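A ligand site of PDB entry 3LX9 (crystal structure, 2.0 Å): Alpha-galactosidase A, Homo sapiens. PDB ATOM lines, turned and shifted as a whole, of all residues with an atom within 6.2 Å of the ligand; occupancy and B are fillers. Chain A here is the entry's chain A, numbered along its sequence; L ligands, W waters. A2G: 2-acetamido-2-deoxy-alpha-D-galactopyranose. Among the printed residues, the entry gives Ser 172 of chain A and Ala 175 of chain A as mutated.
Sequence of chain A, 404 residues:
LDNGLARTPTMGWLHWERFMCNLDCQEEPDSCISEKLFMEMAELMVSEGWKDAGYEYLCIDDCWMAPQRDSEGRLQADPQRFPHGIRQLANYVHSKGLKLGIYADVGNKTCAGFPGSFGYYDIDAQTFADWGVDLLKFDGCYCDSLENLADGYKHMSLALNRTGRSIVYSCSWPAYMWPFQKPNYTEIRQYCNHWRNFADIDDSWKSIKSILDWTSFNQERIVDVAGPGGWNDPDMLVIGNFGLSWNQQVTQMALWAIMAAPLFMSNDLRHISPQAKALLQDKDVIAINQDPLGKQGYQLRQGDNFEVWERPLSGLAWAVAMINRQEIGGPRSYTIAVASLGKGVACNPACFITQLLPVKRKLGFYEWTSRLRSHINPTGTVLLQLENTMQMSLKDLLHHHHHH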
ATOM      1  N   LEU A  14       2.275 -22.068   5.134  1.00  0.00           N
ATOM      2  CA  LEU A  14       2.188 -20.764   5.792  1.00  0.00           C
ATOM      3  C   LEU A  14       3.181 -20.753   6.941  1.00  0.00           C
ATOM      4  O   LEU A  14       3.154 -21.654   7.784  1.00  0.00           O
ATOM      5  CB  LEU A  14       0.754 -20.533   6.290  1.00  0.00           C
ATOM      6  CG  LEU A  14       0.386 -19.221   6.994  1.00  0.00           C
ATOM      7  CD1 LEU A  14       0.705 -17.992   6.130  1.00  0.00           C
ATOM      8  CD2 LEU A  14      -1.085 -19.243   7.353  1.00  0.00           C
ATOM      9  N   TRP A  16       3.773 -19.141   9.723  1.00  0.00           N
ATOM     10  CA  TRP A  16       3.592 -18.527  11.037  1.00  0.00           C
ATOM     11  C   TRP A  16       3.845 -19.416  12.256  1.00  0.00           C
ATOM     12  O   TRP A  16       4.614 -19.055  13.130  1.00  0.00           O
ATOM     13  CB  TRP A  16       2.208 -17.888  11.181  1.00  0.00           C
ATOM     14  CG  TRP A  16       2.119 -17.181  12.488  1.00  0.00           C
ATOM     15  CD1 TRP A  16       1.369 -17.551  13.570  1.00  0.00           C
ATOM     16  CD2 TRP A  16       2.849 -16.013  12.877  1.00  0.00           C
ATOM     17  NE1 TRP A  16       1.573 -16.662  14.600  1.00  0.00           N
ATOM     18  CE2 TRP A  16       2.466 -15.707  14.208  1.00  0.00           C
ATOM     19  CE3 TRP A  16       3.753 -15.186  12.224  1.00  0.00           C
ATOM     20  CZ2 TRP A  16       2.983 -14.605  14.893  1.00  0.00           C
ATOM     21  CZ3 TRP A  16       4.270 -14.084  12.909  1.00  0.00           C
ATOM     22  CH2 TRP A  16       3.879 -13.806  14.234  1.00  0.00           C
ATOM     23  N   ASP A  61       3.297 -14.957   6.061  1.00  0.00           N
ATOM     24  CA  ASP A  61       2.453 -14.435   7.120  1.00  0.00           C
ATOM     25  C   ASP A  61       3.049 -13.096   7.617  1.00  0.00           C
ATOM     26  O   ASP A  61       3.695 -12.391   6.845  1.00  0.00           O
ATOM     27  CB  ASP A  61       2.311 -15.471   8.255  1.00  0.00           C
ATOM     28  CG  ASP A  61       1.020 -15.304   9.034  1.00  0.00           C
ATOM     29  OD1 ASP A  61       1.005 -14.517  10.014  1.00  0.00           O
ATOM     30  OD2 ASP A  61       0.016 -15.964   8.692  1.00  0.00           O
ATOM     31  N   ASP A  62       2.836 -12.752   8.888  1.00  0.00           N
ATOM     32  CA  ASP A  62       3.243 -11.446   9.431  1.00  0.00           C
ATOM     33  C   ASP A  62       4.765 -11.301   9.473  1.00  0.00           C
ATOM     34  O   ASP A  62       5.508 -12.278   9.338  1.00  0.00           O
ATOM     35  CB  ASP A  62       2.640 -11.289  10.833  1.00  0.00           C
ATOM     36  CG  ASP A  62       2.481  -9.844  11.277  1.00  0.00           C
ATOM     37  OD1 ASP A  62       3.029  -8.924  10.628  1.00  0.00           O
ATOM     38  OD2 ASP A  62       1.795  -9.631  12.303  1.00  0.00           O
ATOM     39  N   CYS A  63       5.229 -10.061   9.631  1.00  0.00           N
ATOM     40  CA  CYS A  63       6.656  -9.729   9.811  1.00  0.00           C
ATOM     41  C   CYS A  63       7.511  -9.852   8.544  1.00  0.00           C
ATOM     42  O   CYS A  63       8.691 -10.204   8.608  1.00  0.00           O
ATOM     43  CB  CYS A  63       7.276 -10.547  10.959  1.00  0.00           C
ATOM     44  SG  CYS A  63       6.300 -10.460  12.465  1.00  0.00           S
ATOM     45  N   TYR A 103       0.546 -11.405   3.634  1.00  0.00           N
ATOM     46  CA  TYR A 103      -0.204 -11.033   4.816  1.00  0.00           C
ATOM     47  C   TYR A 103      -0.345  -9.531   4.926  1.00  0.00           C
ATOM     48  O   TYR A 103       0.593  -8.787   4.636  1.00  0.00           O
ATOM     49  CB  TYR A 103       0.507 -11.586   6.048  1.00  0.00           C
ATOM     50  CG  TYR A 103      -0.039 -11.152   7.391  1.00  0.00           C
ATOM     51  CD1 TYR A 103      -0.827 -12.001   8.159  1.00  0.00           C
ATOM     52  CD2 TYR A 103       0.248  -9.894   7.911  1.00  0.00           C
ATOM     53  CE1 TYR A 103      -1.326 -11.607   9.395  1.00  0.00           C
ATOM     54  CE2 TYR A 103      -0.247  -9.493   9.124  1.00  0.00           C
ATOM     55  CZ  TYR A 103      -1.026 -10.356   9.877  1.00  0.00           C
ATOM     56  OH  TYR A 103      -1.515  -9.951  11.096  1.00  0.00           O
ATOM     57  N   THR A 110      -0.325  -4.565  11.995  1.00  0.00           N
ATOM     58  CA  THR A 110      -0.431  -6.016  11.992  1.00  0.00           C
ATOM     59  C   THR A 110      -0.350  -6.481  13.440  1.00  0.00           C
ATOM     60  O   THR A 110      -0.019  -5.683  14.333  1.00  0.00           O
ATOM     61  CB  THR A 110       0.695  -6.680  11.178  1.00  0.00           C
ATOM     62  OG1 THR A 110       1.952  -6.449  11.815  1.00  0.00           O
ATOM     63  CG2 THR A 110       0.744  -6.131   9.754  1.00  0.00           C
ATOM     64  N   CYS A 111      -0.636  -7.756  13.690  1.00  0.00           N
ATOM     65  CA  CYS A 111      -0.617  -8.262  15.070  1.00  0.00           C
ATOM     66  C   CYS A 111       0.789  -8.200  15.672  1.00  0.00           C
ATOM     67  O   CYS A 111       0.936  -7.980  16.864  1.00  0.00           O
ATOM     68  CB  CYS A 111      -1.173  -9.691  15.142  1.00  0.00           C
ATOM     69  SG  CYS A 111      -2.874  -9.835  14.564  1.00  0.00           S
ATOM     70  N   ALA A 112       1.812  -8.369  14.830  1.00  0.00           N
ATOM     71  CA  ALA A 112       3.192  -8.247  15.271  1.00  0.00           C
ATOM     72  C   ALA A 112       3.682  -6.792  15.334  1.00  0.00           C
ATOM     73  O   ALA A 112       4.843  -6.542  15.660  1.00  0.00           O
ATOM     74  CB  ALA A 112       4.105  -9.065  14.358  1.00  0.00           C
ATOM     75  N   LYS A 137      -3.847 -13.049   3.041  1.00  0.00           N
ATOM     76  CA  LYS A 137      -4.397 -13.291   4.368  1.00  0.00           C
ATOM     77  C   LYS A 137      -4.521 -11.939   5.047  1.00  0.00           C
ATOM     78  O   LYS A 137      -3.526 -11.230   5.202  1.00  0.00           O
ATOM     79  CB  LYS A 137      -3.487 -14.224   5.186  1.00  0.00           C
ATOM     80  CG  LYS A 137      -3.921 -14.363   6.656  1.00  0.00           C
ATOM     81  CD  LYS A 137      -3.061 -15.379   7.405  1.00  0.00           C
ATOM     82  CE  LYS A 137      -3.355 -15.332   8.901  1.00  0.00           C
ATOM     83  NZ  LYS A 137      -2.474 -16.237   9.682  1.00  0.00           N
ATOM     84  N   PHE A 138      -5.744 -11.577   5.433  1.00  0.00           N
ATOM     85  CA  PHE A 138      -6.050 -10.241   5.917  1.00  0.00           C
ATOM     86  C   PHE A 138      -6.522 -10.338   7.367  1.00  0.00           C
ATOM     87  O   PHE A 138      -7.600 -10.859   7.650  1.00  0.00           O
ATOM     88  CB  PHE A 138      -7.101  -9.591   5.014  1.00  0.00           C
ATOM     89  CG  PHE A 138      -7.052  -8.076   4.986  1.00  0.00           C
ATOM     90  CD1 PHE A 138      -5.853  -7.388   4.831  1.00  0.00           C
ATOM     91  CD2 PHE A 138      -8.227  -7.333   5.067  1.00  0.00           C
ATOM     92  CE1 PHE A 138      -5.823  -6.004   4.795  1.00  0.00           C
ATOM     93  CE2 PHE A 138      -8.209  -5.941   5.022  1.00  0.00           C
ATOM     94  CZ  PHE A 138      -7.001  -5.276   4.888  1.00  0.00           C
ATOM     95  N   ASP A 139      -5.702  -9.818   8.276  1.00  0.00           N
ATOM     96  CA  ASP A 139      -5.888 -10.004   9.710  1.00  0.00           C
ATOM     97  C   ASP A 139      -6.679  -8.846  10.331  1.00  0.00           C
ATOM     98  O   ASP A 139      -6.827  -7.796   9.708  1.00  0.00           O
ATOM     99  CB  ASP A 139      -4.514 -10.134  10.369  1.00  0.00           C
ATOM    100  CG  ASP A 139      -4.514 -11.039  11.592  1.00  0.00           C
ATOM    101  OD1 ASP A 139      -5.589 -11.293  12.173  1.00  0.00           O
ATOM    102  OD2 ASP A 139      -3.422 -11.503  11.969  1.00  0.00           O
ATOM    103  N   GLY A 140      -7.184  -9.051  11.535  1.00  0.00           N
ATOM    104  CA  GLY A 140      -8.109  -8.103  12.169  1.00  0.00           C
ATOM    105  C   GLY A 140      -7.586  -7.377  13.392  1.00  0.00           C
ATOM    106  O   GLY A 140      -8.369  -6.803  14.153  1.00  0.00           O
ATOM    107  N   CYS A 141      -6.263  -7.383  13.590  1.00  0.00           N
ATOM    108  CA  CYS A 141      -5.661  -6.729  14.754  1.00  0.00           C
ATOM    109  C   CYS A 141      -5.743  -5.206  14.691  1.00  0.00           C
ATOM    110  O   CYS A 141      -5.898  -4.630  13.618  1.00  0.00           O
ATOM    111  CB  CYS A 141      -4.204  -7.147  14.945  1.00  0.00           C
ATOM    112  SG  CYS A 141      -3.980  -8.697  15.831  1.00  0.00           S
ATOM    113  N   SER A 172      -9.826 -12.997   8.519  1.00  0.00           N
ATOM    114  CA  SER A 172      -9.901 -13.336   9.944  1.00  0.00           C
ATOM    115  C   SER A 172     -11.089 -12.634  10.628  1.00  0.00           C
ATOM    116  O   SER A 172     -11.319 -12.821  11.820  1.00  0.00           O
ATOM    117  CB  SER A 172      -8.576 -13.008  10.623  1.00  0.00           C
ATOM    118  OG  SER A 172      -7.521 -13.678   9.966  1.00  0.00           O
ATOM    119  N   ALA A 175     -13.317 -14.329  13.437  1.00  0.00           N
ATOM    120  CA  ALA A 175     -12.521 -14.633  14.646  1.00  0.00           C
ATOM    121  C   ALA A 175     -12.411 -13.437  15.591  1.00  0.00           C
ATOM    122  O   ALA A 175     -12.344 -13.630  16.810  1.00  0.00           O
ATOM    123  CB  ALA A 175     -11.128 -15.139  14.280  1.00  0.00           C
ATOM    124  N   TYR A 176     -12.381 -12.219  15.060  1.00  0.00           N
ATOM    125  CA  TYR A 176     -12.320 -10.993  15.882  1.00  0.00           C
ATOM    126  C   TYR A 176     -13.694 -10.505  16.347  1.00  0.00           C
ATOM    127  O   TYR A 176     -13.773  -9.638  17.219  1.00  0.00           O
ATOM    128  CB  TYR A 176     -11.569  -9.888  15.141  1.00  0.00           C
ATOM    129  CG  TYR A 176     -10.094 -10.198  15.012  1.00  0.00           C
ATOM    130  CD1 TYR A 176      -9.606 -10.920  13.927  1.00  0.00           C
ATOM    131  CD2 TYR A 176      -9.195  -9.818  16.008  1.00  0.00           C
ATOM    132  CE1 TYR A 176      -8.258 -11.227  13.823  1.00  0.00           C
ATOM    133  CE2 TYR A 176      -7.841 -10.120  15.910  1.00  0.00           C
ATOM    134  CZ  TYR A 176      -7.379 -10.833  14.815  1.00  0.00           C
ATOM    135  OH  TYR A 176      -6.045 -11.140  14.708  1.00  0.00           O
ATOM    136  N   ARG A 196     -10.905 -17.375   9.097  1.00  0.00           N
ATOM    137  CA  ARG A 196     -10.531 -17.861  10.420  1.00  0.00           C
ATOM    138  C   ARG A 196     -11.654 -17.552  11.418  1.00  0.00           C
ATOM    139  O   ARG A 196     -12.064 -16.400  11.543  1.00  0.00           O
ATOM    140  CB  ARG A 196      -9.224 -17.207  10.872  1.00  0.00           C
ATOM    141  CG  ARG A 196      -7.981 -17.750  10.159  1.00  0.00           C
ATOM    142  CD  ARG A 196      -7.505 -19.059  10.770  1.00  0.00           C
ATOM    143  NE  ARG A 196      -7.415 -18.960  12.223  1.00  0.00           N
ATOM    144  CZ  ARG A 196      -6.443 -18.356  12.896  1.00  0.00           C
ATOM    145  NH1 ARG A 196      -5.411 -17.804  12.263  1.00  0.00           N
ATOM    146  NH2 ARG A 196      -6.486 -18.317  14.224  1.00  0.00           N
ATOM    147  N   PHE A 198     -11.569 -18.941  14.842  1.00  0.00           N
ATOM    148  CA  PHE A 198     -11.205 -19.206  16.233  1.00  0.00           C
ATOM    149  C   PHE A 198      -9.726 -18.871  16.527  1.00  0.00           C
ATOM    150  O   PHE A 198      -8.999 -18.438  15.636  1.00  0.00           O
ATOM    151  CB  PHE A 198     -11.562 -20.667  16.557  1.00  0.00           C
ATOM    152  CG  PHE A 198     -11.501 -21.011  18.024  1.00  0.00           C
ATOM    153  CD1 PHE A 198     -12.271 -20.311  18.950  1.00  0.00           C
ATOM    154  CD2 PHE A 198     -10.668 -22.035  18.475  1.00  0.00           C
ATOM    155  CE1 PHE A 198     -12.197 -20.616  20.306  1.00  0.00           C
ATOM    156  CE2 PHE A 198     -10.601 -22.353  19.830  1.00  0.00           C
ATOM    157  CZ  PHE A 198     -11.377 -21.649  20.744  1.00  0.00           C
ATOM    158  N   ALA A 199      -9.328 -19.050  17.790  1.00  0.00           N
ATOM    159  CA  ALA A 199      -7.980 -18.709  18.260  1.00  0.00           C
ATOM    160  C   ALA A 199      -6.863 -19.403  17.487  1.00  0.00           C
ATOM    161  O   ALA A 199      -7.051 -20.477  16.898  1.00  0.00           O
ATOM    162  CB  ALA A 199      -7.859 -19.043  19.754  1.00  0.00           C
ATOM    163  N   ASP A 200      -5.689 -18.767  17.507  1.00  0.00           N
ATOM    164  CA  ASP A 200      -4.496 -19.280  16.836  1.00  0.00           C
ATOM    165  C   ASP A 200      -4.152 -20.675  17.324  1.00  0.00           C
ATOM    166  O   ASP A 200      -4.136 -20.935  18.526  1.00  0.00           O
ATOM    167  CB  ASP A 200      -3.302 -18.360  17.096  1.00  0.00           C
ATOM    168  CG  ASP A 200      -3.429 -17.001  16.430  1.00  0.00           C
ATOM    169  OD1 ASP A 200      -4.419 -16.767  15.696  1.00  0.00           O
ATOM    170  OD2 ASP A 200      -2.540 -16.160  16.648  1.00  0.00           O
ATOM    171  N   ASP A 235      -7.504 -23.098  11.128  1.00  0.00           N
ATOM    172  CA  ASP A 235      -6.078 -22.728  11.240  1.00  0.00           C
ATOM    173  C   ASP A 235      -5.130 -23.842  10.760  1.00  0.00           C
ATOM    174  O   ASP A 235      -5.574 -24.885  10.284  1.00  0.00           O
ATOM    175  CB  ASP A 235      -5.719 -22.227  12.647  1.00  0.00           C
ATOM    176  CG  ASP A 235      -4.616 -21.167  12.637  1.00  0.00           C
ATOM    177  OD1 ASP A 235      -4.056 -20.877  11.556  1.00  0.00           O
ATOM    178  OD2 ASP A 235      -4.299 -20.630  13.718  1.00  0.00           O
ATOM    179  N   MET A 236      -3.833 -23.584  10.881  1.00  0.00           N
ATOM    180  CA  MET A 236      -2.796 -24.384  10.217  1.00  0.00           C
ATOM    181  C   MET A 236      -2.695 -25.833  10.678  1.00  0.00           C
ATOM    182  O   MET A 236      -3.029 -26.168  11.818  1.00  0.00           O
ATOM    183  CB  MET A 236      -1.441 -23.715  10.436  1.00  0.00           C
ATOM    184  CG  MET A 236      -1.270 -22.382   9.705  1.00  0.00           C
ATOM    185  SD  MET A 236       0.000 -21.334  10.429  1.00  0.00           S
ATOM    186  CE  MET A 236      -0.871 -20.715  11.870  1.00  0.00           C
HETATM  187  O5  A2G L   1      -1.474 -12.781  13.917  1.00  0.00           O
HETATM  188  C1  A2G L   1      -2.722 -13.375  14.298  1.00  0.00           C
HETATM  189  O1  A2G L   1      -3.027 -13.541  15.681  1.00  0.00           O
HETATM  190  C2  A2G L   1      -3.282 -14.407  13.297  1.00  0.00           C
HETATM  191  N2  A2G L   1      -4.600 -14.874  13.695  1.00  0.00           N
HETATM  192  C3  A2G L   1      -2.239 -15.508  13.138  1.00  0.00           C
HETATM  193  O3  A2G L   1      -2.716 -16.534  12.280  1.00  0.00           O
HETATM  194  C4  A2G L   1      -0.967 -14.837  12.598  1.00  0.00           C
HETATM  195  O4  A2G L   1      -1.247 -14.310  11.283  1.00  0.00           O
HETATM  196  C5  A2G L   1      -0.448 -13.723  13.529  1.00  0.00           C
HETATM  197  C6  A2G L   1       0.661 -12.926  12.883  1.00  0.00           C
HETATM  198  O6  A2G L   1       1.205 -11.962  13.792  1.00  0.00           O
HETATM  199  C7  A2G L   1      -5.690 -14.668  12.951  1.00  0.00           C
HETATM  200  O7  A2G L   1      -5.641 -14.187  11.836  1.00  0.00           O
HETATM  201  C8  A2G L   1      -7.013 -15.010  13.576  1.00  0.00           C
HETATM  202  O   HOH W   1      -2.478 -18.666  13.687  1.00  0.00           O
HETATM  203  O   HOH W   2      -5.141 -12.179  16.939  1.00  0.00           O
HETATM  204  O   HOH W   3       1.763 -11.783  16.330  1.00  0.00           O
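OD2 of Asp 62 sits at hydrogen-bond distance from O6 of the ligand, at 2.8 Å.
The side-chain carboxylate (OD1) of Asp 200 sits at hydrogen-bond distance from a nitrogen (N2) of the ligand (2.8 Å).
The side-chain hydroxyl of Ser 172 is in hydrogen-bond range of an oxygen (O7) of the ligand, at 2.7 Å.
The guanidinium group of Arg 196 is in hydrogen-bond range of an oxygen (O3) of the ligand (3.0 Å).
The side-chain carboxylate (OD1) of Asp 61 is in hydrogen-bond range of an oxygen (O4) of the ligand (2.6 Å).
An oxygen (O3) of the ligand lies within hydrogen-bond range of the side-chain amino group (NZ) of Lys 137 (2.6 Å).
The backbone carbonyl oxygen (O) of Ala 199 sits close to the guanidinium group (NH2) of Arg 196 (3.5 Å).
N of Cys 111 is in hydrogen-bond range of OD2 of Asp 62.
NZ of Lys 137 is in salt-bridge range of OD2 of Asp 61, at 2.7 Å.
The backbone carbonyl oxygen (O) of Phe 198 is in hydrogen-bond range of the guanidinium group (NH2) of Arg 196.
The side-chain carboxylate of Asp 139 is in hydrogen-bond range of the side-chain hydroxyl of Tyr 103 (2.6 Å).
The side-chain carboxylate of Asp 62 lies within hydrogen-bond range of the backbone NH of Ala 112, at 2.8 Å.
The side-chain hydroxyl (OH) of Tyr 176 is in hydrogen-bond range of the side-chain sulfur (SG) of Cys 111 (3.4 Å).
SG of Cys 111 forms a disulfide with SG of Cys 141 (2.0 Å).
The side-chain sulfur (SG) of Cys 111 sits close to an oxygen (O5) of the ligand, 3.3 Å away.
The side-chain carboxylate (OD1) of Asp 139 sits close to an oxygen (O7) of the ligand (2.9 Å).
Trp 16 touches the ligand.
CE1 of Tyr 103 touches O4 of the ligand, 3.3 Å away.
Ala 112 touches the ligand.
Tyr 176 touches the ligand (OH to C7, 3.96 Å).
12 residues have an atom within 4 Å of the ligand: Trp 16, Asp 61, Asp 62, Tyr 103, Cys 111, Ala 112, Lys 137, Asp 139, Ser 172, Tyr 176, Arg 196 and Asp 200.
Along chain A the residues within 4 Å of the ligand span positions 16 to 200.
The nearest printed residue that does not touch the ligand is Ala 175 (4.2 Å).
Water W1 lies within hydrogen-bond range of O3 of the ligand (2.6 Å), OD2 of Asp 235 (2.7 Å), NH1 of Arg 196 (3.4 Å) and OD1 of Asp 200 (3.4 Å).
Water W2 lies within hydrogen-bond range of OH of Tyr 176 (2.6 Å) and O1 of the ligand (2.8 Å).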
